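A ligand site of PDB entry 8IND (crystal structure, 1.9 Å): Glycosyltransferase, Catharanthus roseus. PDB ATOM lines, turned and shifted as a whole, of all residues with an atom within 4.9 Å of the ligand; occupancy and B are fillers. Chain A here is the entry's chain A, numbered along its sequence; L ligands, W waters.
A nitrogen (N2) of the ligand lies close to the indole nitrogen of Trp 340 (3.4 Å). CA of Gly 15 touches O10 of the ligand, 3.5 Å away. OH of Tyr 282 touches O2 of the ligand (3.8 Å). Ser 284 touches the ligand. C of Gly 286 touches O12 of the ligand, 3.8 Å away. Val 313 touches the ligand. Gly 360 touches the ligand (C to O7, 3.7 Å).
The side-chain amide oxygen (OE1) of Gln 343 lies within hydrogen-bond range of the side-chain hydroxyl (OG) of Ser 363 (3.0 Å). The side-chain hydroxyl of Tyr 282 lies within hydrogen-bond range of the side-chain amide nitrogen of Gln 343, 2.7 Å away. ND2 of Asn 18 lies close to O of Lys 14 (3.5 Å). The side-chain carboxylate of Glu 366 lies close to the side-chain amide oxygen of Gln 343 (2.8 Å). The side-chain hydroxyl (OH) of Tyr 282 lies within hydrogen-bond range of the side-chain sulfur (SG) of Cys 341 (3.1 Å). The side-chain amide nitrogen (ND2) of Asn 362 lies within hydrogen-bond range of the backbone carbonyl oxygen (O) of Gly 15, at 2.8 Å. The backbone NH of Gly 286 sits at hydrogen-bond distance from the side-chain hydroxyl of Ser 284, 3.2 Å away. O of Ser 284 lies within hydrogen-bond range of N of His 358, at 3.4 Å.
Water W6 lies within hydrogen-bond range of O11 of the ligand (2.7 Å), N of Leu 288 (2.9 Å), NE2 of His 358 (3.2 Å) and N of Ser 287 (3.3 Å). Water W2 lies within hydrogen-bond range of O10 of the ligand (2.7 Å), N of Gly 15 (2.8 Å), OG of Ser 287 (3.2 Å) and N of Lys 14 (3.5 Å). Water W4 bridges the side-chain carboxylate of Glu 366 (2.7 Å) and an oxygen (O5) of the ligand (2.8 Å). Water W3 lies within hydrogen-bond range of O1 of the ligand (3.0 Å), NE1 of Trp 340 (3.1 Å) and ND2 of Asn 18 (3.1 Å). Water W7 lies within hydrogen-bond range of OG of Ser 284, NE2 of Gln 343 and OG of Ser 363.
A ring nitrogen (NE2) of His 358 is in hydrogen-bond range of an oxygen (O11) of the ligand (3.0 Å). The side-chain carboxylate (OE1) of Glu 366 is in hydrogen-bond range of an oxygen (O3) of the ligand. ND2 of Asn 362 is in hydrogen-bond range of O7 of the ligand. An oxygen (O2) of the ligand is in hydrogen-bond range of the side-chain sulfur (SG) of Cys 341 (3.4 Å). O of Cys 341 lies within hydrogen-bond range of N2 of the ligand (2.8 Å). An oxygen (O7) of the ligand lies within hydrogen-bond range of the backbone NH of Asn 362 (3.1 Å). The backbone NH of Trp 361 lies within hydrogen-bond range of an oxygen (O7) of the ligand, 3.4 Å away. OG of Ser 287 sits at hydrogen-bond distance from O12 of the ligand, at 2.6 Å. OG of Ser 363 sits at hydrogen-bond distance from O8 of the ligand, at 2.7 Å. O3 of the ligand is in hydrogen-bond range of OE1 of Gln 343. ND2 of Asn 18 sits at hydrogen-bond distance from O5 of the ligand, at 3.2 Å. O8 of the ligand is in hydrogen-bond range of N of Ser 363 (2.9 Å). N of Cys 341 lies within hydrogen-bond range of O2 of the ligand (2.8 Å). An oxygen (O12) of the ligand lies within hydrogen-bond range of the backbone NH of Ser 287 (2.8 Å).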
ATOM      1  N   LYS A  14     -13.141  19.778   4.540  1.00  0.00           N
ATOM      2  CA  LYS A  14     -13.546  21.186   4.643  1.00  0.00           C
ATOM      3  C   LYS A  14     -14.481  21.450   5.831  1.00  0.00           C
ATOM      4  O   LYS A  14     -14.373  22.507   6.464  1.00  0.00           O
ATOM      5  CB  LYS A  14     -14.169  21.655   3.320  1.00  0.00           C
ATOM      6  CG  LYS A  14     -13.053  21.982   2.337  1.00  0.00           C
ATOM      7  CD  LYS A  14     -13.547  22.439   0.972  1.00  0.00           C
ATOM      8  CE  LYS A  14     -12.416  22.421  -0.064  1.00  0.00           C
ATOM      9  NZ  LYS A  14     -11.563  21.203   0.024  1.00  0.00           N
ATOM     10  N   GLY A  15     -15.372  20.517   6.161  1.00  0.00           N
ATOM     11  CA  GLY A  15     -16.224  20.710   7.338  1.00  0.00           C
ATOM     12  C   GLY A  15     -15.480  20.638   8.664  1.00  0.00           C
ATOM     13  O   GLY A  15     -16.065  20.926   9.716  1.00  0.00           O
ATOM     14  N   ASN A  18     -12.769  24.324   8.162  1.00  0.00           N
ATOM     15  CA  ASN A  18     -13.394  25.648   8.207  1.00  0.00           C
ATOM     16  C   ASN A  18     -13.815  26.083   9.611  1.00  0.00           C
ATOM     17  O   ASN A  18     -13.512  27.227   9.991  1.00  0.00           O
ATOM     18  CB  ASN A  18     -14.575  25.680   7.217  1.00  0.00           C
ATOM     19  CG  ASN A  18     -14.122  25.675   5.776  1.00  0.00           C
ATOM     20  OD1 ASN A  18     -12.938  25.808   5.494  1.00  0.00           O
ATOM     21  ND2 ASN A  18     -15.066  25.506   4.848  1.00  0.00           N
ATOM     22  N   TYR A 259     -12.052  32.593   3.955  1.00  0.00           N
ATOM     23  CA  TYR A 259     -12.016  31.400   3.093  1.00  0.00           C
ATOM     24  C   TYR A 259     -10.585  31.043   2.696  1.00  0.00           C
ATOM     25  O   TYR A 259      -9.784  31.935   2.421  1.00  0.00           O
ATOM     26  CB  TYR A 259     -12.914  31.563   1.865  1.00  0.00           C
ATOM     27  CG  TYR A 259     -14.314  32.023   2.150  1.00  0.00           C
ATOM     28  CD1 TYR A 259     -15.262  31.157   2.675  1.00  0.00           C
ATOM     29  CD2 TYR A 259     -14.704  33.329   1.902  1.00  0.00           C
ATOM     30  CE1 TYR A 259     -16.552  31.572   2.956  1.00  0.00           C
ATOM     31  CE2 TYR A 259     -15.992  33.768   2.182  1.00  0.00           C
ATOM     32  CZ  TYR A 259     -16.913  32.883   2.709  1.00  0.00           C
ATOM     33  OH  TYR A 259     -18.185  33.290   2.976  1.00  0.00           O
ATOM     34  N   THR A 263     -13.703  30.352  -3.772  1.00  0.00           N
ATOM     35  CA  THR A 263     -15.135  30.461  -3.516  1.00  0.00           C
ATOM     36  C   THR A 263     -15.900  31.198  -4.606  1.00  0.00           C
ATOM     37  O   THR A 263     -17.121  31.348  -4.465  1.00  0.00           O
ATOM     38  CB  THR A 263     -15.373  31.177  -2.174  1.00  0.00           C
ATOM     39  OG1 THR A 263     -14.668  32.424  -2.179  1.00  0.00           O
ATOM     40  CG2 THR A 263     -14.902  30.296  -1.007  1.00  0.00           C
ATOM     41  N   TYR A 282     -30.894  28.469  -2.221  1.00  0.00           N
ATOM     42  CA  TYR A 282     -29.488  28.061  -2.216  1.00  0.00           C
ATOM     43  C   TYR A 282     -29.459  26.542  -2.043  1.00  0.00           C
ATOM     44  O   TYR A 282     -30.200  26.005  -1.218  1.00  0.00           O
ATOM     45  CB  TYR A 282     -28.737  28.778  -1.095  1.00  0.00           C
ATOM     46  CG  TYR A 282     -27.313  28.306  -0.870  1.00  0.00           C
ATOM     47  CD1 TYR A 282     -26.446  28.115  -1.944  1.00  0.00           C
ATOM     48  CD2 TYR A 282     -26.854  28.068   0.415  1.00  0.00           C
ATOM     49  CE1 TYR A 282     -25.127  27.667  -1.721  1.00  0.00           C
ATOM     50  CE2 TYR A 282     -25.550  27.622   0.640  1.00  0.00           C
ATOM     51  CZ  TYR A 282     -24.696  27.433  -0.432  1.00  0.00           C
ATOM     52  OH  TYR A 282     -23.403  26.989  -0.188  1.00  0.00           O
ATOM     53  N   SER A 284     -26.896  23.113  -1.730  1.00  0.00           N
ATOM     54  CA  SER A 284     -25.538  22.595  -1.617  1.00  0.00           C
ATOM     55  C   SER A 284     -25.548  21.315  -0.794  1.00  0.00           C
ATOM     56  O   SER A 284     -26.231  21.240   0.234  1.00  0.00           O
ATOM     57  CB  SER A 284     -24.591  23.624  -0.982  1.00  0.00           C
ATOM     58  OG  SER A 284     -23.314  23.040  -0.685  1.00  0.00           O
ATOM     59  N   GLY A 286     -22.622  20.113   0.340  1.00  0.00           N
ATOM     60  CA  GLY A 286     -21.389  20.152   1.091  1.00  0.00           C
ATOM     61  C   GLY A 286     -20.167  19.778   0.271  1.00  0.00           C
ATOM     62  O   GLY A 286     -20.144  19.827  -0.960  1.00  0.00           O
ATOM     63  N   SER A 287     -19.110  19.396   1.000  1.00  0.00           N
ATOM     64  CA  SER A 287     -17.774  19.167   0.439  1.00  0.00           C
ATOM     65  C   SER A 287     -17.506  17.704   0.096  1.00  0.00           C
ATOM     66  O   SER A 287     -16.538  17.426  -0.618  1.00  0.00           O
ATOM     67  CB  SER A 287     -16.694  19.685   1.421  1.00  0.00           C
ATOM     68  OG  SER A 287     -16.556  18.824   2.557  1.00  0.00           O
ATOM     69  N   LEU A 288     -18.333  16.777   0.563  1.00  0.00           N
ATOM     70  CA  LEU A 288     -18.034  15.352   0.541  1.00  0.00           C
ATOM     71  C   LEU A 288     -19.108  14.540  -0.161  1.00  0.00           C
ATOM     72  O   LEU A 288     -18.788  13.666  -0.974  1.00  0.00           O
ATOM     73  CB  LEU A 288     -17.885  14.860   1.983  1.00  0.00           C
ATOM     74  CG  LEU A 288     -16.594  15.208   2.725  1.00  0.00           C
ATOM     75  CD1 LEU A 288     -16.539  14.391   3.990  1.00  0.00           C
ATOM     76  CD2 LEU A 288     -15.347  14.962   1.869  1.00  0.00           C
ATOM     77  N   VAL A 313     -24.504  24.788  -5.768  1.00  0.00           N
ATOM     78  CA  VAL A 313     -23.098  24.385  -5.717  1.00  0.00           C
ATOM     79  C   VAL A 313     -23.000  22.938  -6.157  1.00  0.00           C
ATOM     80  O   VAL A 313     -23.473  22.036  -5.459  1.00  0.00           O
ATOM     81  CB  VAL A 313     -22.518  24.570  -4.302  1.00  0.00           C
ATOM     82  CG1 VAL A 313     -21.069  24.023  -4.231  1.00  0.00           C
ATOM     83  CG2 VAL A 313     -22.557  26.021  -3.906  1.00  0.00           C
ATOM     84  N   TRP A 340     -18.237  26.111  -6.247  1.00  0.00           N
ATOM     85  CA  TRP A 340     -18.050  26.444  -4.834  1.00  0.00           C
ATOM     86  C   TRP A 340     -18.433  27.913  -4.684  1.00  0.00           C
ATOM     87  O   TRP A 340     -18.217  28.700  -5.604  1.00  0.00           O
ATOM     88  CB  TRP A 340     -16.579  26.206  -4.387  1.00  0.00           C
ATOM     89  CG  TRP A 340     -16.387  25.891  -2.897  1.00  0.00           C
ATOM     90  CD1 TRP A 340     -15.666  26.620  -1.988  1.00  0.00           C
ATOM     91  CD2 TRP A 340     -16.879  24.750  -2.179  1.00  0.00           C
ATOM     92  NE1 TRP A 340     -15.698  26.006  -0.744  1.00  0.00           N
ATOM     93  CE2 TRP A 340     -16.449  24.859  -0.839  1.00  0.00           C
ATOM     94  CE3 TRP A 340     -17.678  23.656  -2.543  1.00  0.00           C
ATOM     95  CZ2 TRP A 340     -16.771  23.917   0.129  1.00  0.00           C
ATOM     96  CZ3 TRP A 340     -17.992  22.710  -1.570  1.00  0.00           C
ATOM     97  CH2 TRP A 340     -17.546  22.865  -0.251  1.00  0.00           C
ATOM     98  N   CYS A 341     -19.012  28.262  -3.540  1.00  0.00           N
ATOM     99  CA  CYS A 341     -19.466  29.620  -3.289  1.00  0.00           C
ATOM    100  C   CYS A 341     -18.948  30.097  -1.947  1.00  0.00           C
ATOM    101  O   CYS A 341     -18.414  29.305  -1.159  1.00  0.00           O
ATOM    102  CB  CYS A 341     -21.000  29.705  -3.314  1.00  0.00           C
ATOM    103  SG  CYS A 341     -21.846  29.073  -1.864  1.00  0.00           S
ATOM    104  N   PRO A 342     -19.042  31.398  -1.656  1.00  0.00           N
ATOM    105  CA  PRO A 342     -18.692  31.849  -0.311  1.00  0.00           C
ATOM    106  C   PRO A 342     -19.896  31.657   0.607  1.00  0.00           C
ATOM    107  O   PRO A 342     -20.734  32.548   0.733  1.00  0.00           O
ATOM    108  CB  PRO A 342     -18.307  33.323  -0.517  1.00  0.00           C
ATOM    109  CG  PRO A 342     -19.188  33.761  -1.706  1.00  0.00           C
ATOM    110  CD  PRO A 342     -19.345  32.524  -2.568  1.00  0.00           C
ATOM    111  N   GLN A 343     -20.002  30.476   1.237  1.00  0.00           N
ATOM    112  CA  GLN A 343     -21.285  30.074   1.797  1.00  0.00           C
ATOM    113  C   GLN A 343     -21.762  31.030   2.890  1.00  0.00           C
ATOM    114  O   GLN A 343     -22.965  31.281   3.021  1.00  0.00           O
ATOM    115  CB  GLN A 343     -21.224  28.623   2.321  1.00  0.00           C
ATOM    116  CG  GLN A 343     -22.457  28.251   3.188  1.00  0.00           C
ATOM    117  CD  GLN A 343     -22.712  26.744   3.328  1.00  0.00           C
ATOM    118  OE1 GLN A 343     -22.885  26.236   4.457  1.00  0.00           O
ATOM    119  NE2 GLN A 343     -22.769  26.038   2.218  1.00  0.00           N
ATOM    120  N   LEU A 344     -20.840  31.548   3.720  1.00  0.00           N
ATOM    121  CA  LEU A 344     -21.263  32.500   4.746  1.00  0.00           C
ATOM    122  C   LEU A 344     -21.901  33.725   4.111  1.00  0.00           C
ATOM    123  O   LEU A 344     -22.947  34.213   4.569  1.00  0.00           O
ATOM    124  CB  LEU A 344     -20.082  32.911   5.615  1.00  0.00           C
ATOM    125  CG  LEU A 344     -19.370  31.767   6.342  1.00  0.00           C
ATOM    126  CD1 LEU A 344     -18.223  32.326   7.202  1.00  0.00           C
ATOM    127  CD2 LEU A 344     -20.369  30.989   7.176  1.00  0.00           C
ATOM    128  N   HIS A 358     -27.660  19.240   2.649  1.00  0.00           N
ATOM    129  CA  HIS A 358     -27.464  17.879   3.138  1.00  0.00           C
ATOM    130  C   HIS A 358     -27.438  17.807   4.666  1.00  0.00           C
ATOM    131  O   HIS A 358     -27.399  16.693   5.203  1.00  0.00           O
ATOM    132  CB  HIS A 358     -26.152  17.286   2.565  1.00  0.00           C
ATOM    133  CG  HIS A 358     -24.904  17.797   3.224  1.00  0.00           C
ATOM    134  ND1 HIS A 358     -24.645  19.139   3.390  1.00  0.00           N
ATOM    135  CD2 HIS A 358     -23.819  17.139   3.697  1.00  0.00           C
ATOM    136  CE1 HIS A 358     -23.467  19.293   3.967  1.00  0.00           C
ATOM    137  NE2 HIS A 358     -22.948  18.097   4.170  1.00  0.00           N
ATOM    138  N   GLY A 360     -25.125  18.827   6.881  1.00  0.00           N
ATOM    139  CA  GLY A 360     -23.882  18.824   7.638  1.00  0.00           C
ATOM    140  C   GLY A 360     -23.937  19.867   8.734  1.00  0.00           C
ATOM    141  O   GLY A 360     -24.691  20.835   8.642  1.00  0.00           O
ATOM    142  N   TRP A 361     -23.168  19.663   9.807  1.00  0.00           N
ATOM    143  CA  TRP A 361     -23.363  20.537  10.969  1.00  0.00           C
ATOM    144  C   TRP A 361     -22.995  21.992  10.667  1.00  0.00           C
ATOM    145  O   TRP A 361     -23.704  22.901  11.112  1.00  0.00           O
ATOM    146  CB  TRP A 361     -22.596  20.056  12.206  1.00  0.00           C
ATOM    147  CG  TRP A 361     -22.854  21.026  13.352  1.00  0.00           C
ATOM    148  CD1 TRP A 361     -21.924  21.731  14.043  1.00  0.00           C
ATOM    149  CD2 TRP A 361     -24.139  21.401  13.896  1.00  0.00           C
ATOM    150  NE1 TRP A 361     -22.543  22.517  14.997  1.00  0.00           N
ATOM    151  CE2 TRP A 361     -23.900  22.342  14.921  1.00  0.00           C
ATOM    152  CE3 TRP A 361     -25.465  21.024  13.615  1.00  0.00           C
ATOM    153  CZ2 TRP A 361     -24.928  22.909  15.679  1.00  0.00           C
ATOM    154  CZ3 TRP A 361     -26.499  21.612  14.362  1.00  0.00           C
ATOM    155  CH2 TRP A 361     -26.220  22.540  15.375  1.00  0.00           C
ATOM    156  N   ASN A 362     -21.912  22.241   9.907  1.00  0.00           N
ATOM    157  CA  ASN A 362     -21.564  23.633   9.615  1.00  0.00           C
ATOM    158  C   ASN A 362     -22.674  24.310   8.823  1.00  0.00           C
ATOM    159  O   ASN A 362     -23.042  25.457   9.089  1.00  0.00           O
ATOM    160  CB  ASN A 362     -20.259  23.732   8.824  1.00  0.00           C
ATOM    161  CG  ASN A 362     -19.074  23.286   9.646  1.00  0.00           C
ATOM    162  OD1 ASN A 362     -18.657  23.968  10.579  1.00  0.00           O
ATOM    163  ND2 ASN A 362     -18.532  22.116   9.302  1.00  0.00           N
ATOM    164  N   SER A 363     -23.211  23.618   7.815  1.00  0.00           N
ATOM    165  CA  SER A 363     -24.260  24.222   7.004  1.00  0.00           C
ATOM    166  C   SER A 363     -25.519  24.472   7.821  1.00  0.00           C
ATOM    167  O   SER A 363     -26.177  25.513   7.678  1.00  0.00           O
ATOM    168  CB  SER A 363     -24.550  23.313   5.800  1.00  0.00           C
ATOM    169  OG  SER A 363     -23.443  23.348   4.895  1.00  0.00           O
ATOM    170  N   GLU A 366     -24.641  27.425  10.237  1.00  0.00           N
ATOM    171  CA  GLU A 366     -24.510  28.668   9.485  1.00  0.00           C
ATOM    172  C   GLU A 366     -25.876  29.161   9.005  1.00  0.00           C
ATOM    173  O   GLU A 366     -26.163  30.360   9.052  1.00  0.00           O
ATOM    174  CB  GLU A 366     -23.541  28.479   8.319  1.00  0.00           C
ATOM    175  CG  GLU A 366     -22.058  28.306   8.792  1.00  0.00           C
ATOM    176  CD  GLU A 366     -21.131  27.661   7.759  1.00  0.00           C
ATOM    177  OE1 GLU A 366     -21.540  27.508   6.592  1.00  0.00           O
ATOM    178  OE2 GLU A 366     -19.977  27.291   8.123  1.00  0.00           O
ATOM    179  N   TRP A 380     -25.860  11.008   5.070  1.00  0.00           N
ATOM    180  CA  TRP A 380     -25.244   9.986   5.921  1.00  0.00           C
ATOM    181  C   TRP A 380     -24.625  10.657   7.156  1.00  0.00           C
ATOM    182  O   TRP A 380     -24.697  11.873   7.329  1.00  0.00           O
ATOM    183  CB  TRP A 380     -24.191   9.161   5.159  1.00  0.00           C
ATOM    184  CG  TRP A 380     -23.401   9.914   4.100  1.00  0.00           C
ATOM    185  CD1 TRP A 380     -23.520   9.793   2.730  1.00  0.00           C
ATOM    186  CD2 TRP A 380     -22.373  10.881   4.320  1.00  0.00           C
ATOM    187  NE1 TRP A 380     -22.620  10.627   2.103  1.00  0.00           N
ATOM    188  CE2 TRP A 380     -21.911  11.310   3.067  1.00  0.00           C
ATOM    189  CE3 TRP A 380     -21.809  11.432   5.479  1.00  0.00           C
ATOM    190  CZ2 TRP A 380     -20.904  12.254   2.923  1.00  0.00           C
ATOM    191  CZ3 TRP A 380     -20.794  12.371   5.340  1.00  0.00           C
ATOM    192  CH2 TRP A 380     -20.351  12.777   4.072  1.00  0.00           C
ATOM    193  N   GLN A 383     -25.822  13.822   9.498  1.00  0.00           N
ATOM    194  CA  GLN A 383     -26.807  14.597   8.738  1.00  0.00           C
ATOM    195  C   GLN A 383     -28.228  14.139   9.039  1.00  0.00           C
ATOM    196  O   GLN A 383     -29.164  14.955   9.054  1.00  0.00           O
ATOM    197  CB  GLN A 383     -26.504  14.492   7.239  1.00  0.00           C
ATOM    198  CG  GLN A 383     -25.137  15.076   6.855  1.00  0.00           C
ATOM    199  CD  GLN A 383     -24.519  14.424   5.642  1.00  0.00           C
ATOM    200  OE1 GLN A 383     -25.214  13.944   4.753  1.00  0.00           O
ATOM    201  NE2 GLN A 383     -23.189  14.385   5.610  1.00  0.00           N
HETATM  202  N1  LIG L   1     -19.007  25.599   1.965  1.00  0.00           N
HETATM  203  C1  LIG L   1     -18.562  26.619   1.280  1.00  0.00           C
HETATM  204  N2  LIG L   1     -18.910  26.833   0.032  1.00  0.00           N
HETATM  205  C2  LIG L   1     -19.735  25.976  -0.555  1.00  0.00           C
HETATM  206  C3  LIG L   1     -20.242  24.876   0.123  1.00  0.00           C
HETATM  207  C4  LIG L   1     -19.835  24.699   1.444  1.00  0.00           C
HETATM  208  O1  LIG L   1     -17.700  27.545   1.860  1.00  0.00           O
HETATM  209  O2  LIG L   1     -20.084  26.216  -1.880  1.00  0.00           O
HETATM  210  C5  LIG L   1     -18.524  25.390   3.344  1.00  0.00           C
HETATM  211  C6  LIG L   1     -19.580  25.554   4.430  1.00  0.00           C
HETATM  212  O3  LIG L   1     -19.607  26.871   4.822  1.00  0.00           O
HETATM  213  C7  LIG L   1     -19.022  24.597   5.516  1.00  0.00           C
HETATM  214  C8  LIG L   1     -18.434  23.592   4.869  1.00  0.00           C
HETATM  215  O4  LIG L   1     -18.083  24.137   3.403  1.00  0.00           O
HETATM  216  O5  LIG L   1     -17.960  25.334   6.244  1.00  0.00           O
HETATM  217  C9  LIG L   1     -19.325  22.389   4.703  1.00  0.00           C
HETATM  218  O6  LIG L   1     -19.377  21.810   5.973  1.00  0.00           O
HETATM  219  P1  LIG L   1     -20.627  20.841   6.440  1.00  0.00           P
HETATM  220  O7  LIG L   1     -20.436  20.459   7.885  1.00  0.00           O
HETATM  221  O8  LIG L   1     -21.911  21.573   6.217  1.00  0.00           O
HETATM  222  O9  LIG L   1     -20.688  19.517   5.513  1.00  0.00           O
HETATM  223  P2  LIG L   1     -19.476  18.558   4.958  1.00  0.00           P
HETATM  224  O10 LIG L   1     -18.477  18.342   6.083  1.00  0.00           O
HETATM  225  O11 LIG L   1     -20.148  17.254   4.649  1.00  0.00           O
HETATM  226  O12 LIG L   1     -18.824  19.173   3.765  1.00  0.00           O
HETATM  227  O   HOH W   1     -17.667  28.912   4.344  1.00  0.00           O
HETATM  228  O   HOH W   2     -15.880  17.866   5.535  1.00  0.00           O
HETATM  229  O   HOH W   3     -14.790  26.847   2.045  1.00  0.00           O
HETATM  230  O   HOH W   4     -17.615  27.945   7.060  1.00  0.00           O
HETATM  231  O   HOH W   5     -19.366  15.191   6.495  1.00  0.00           O
HETATM  232  O   HOH W   6     -20.838  16.772   2.112  1.00  0.00           O
HETATM  233  O   HOH W   7     -22.747  23.287   1.992  1.00  0.00           O
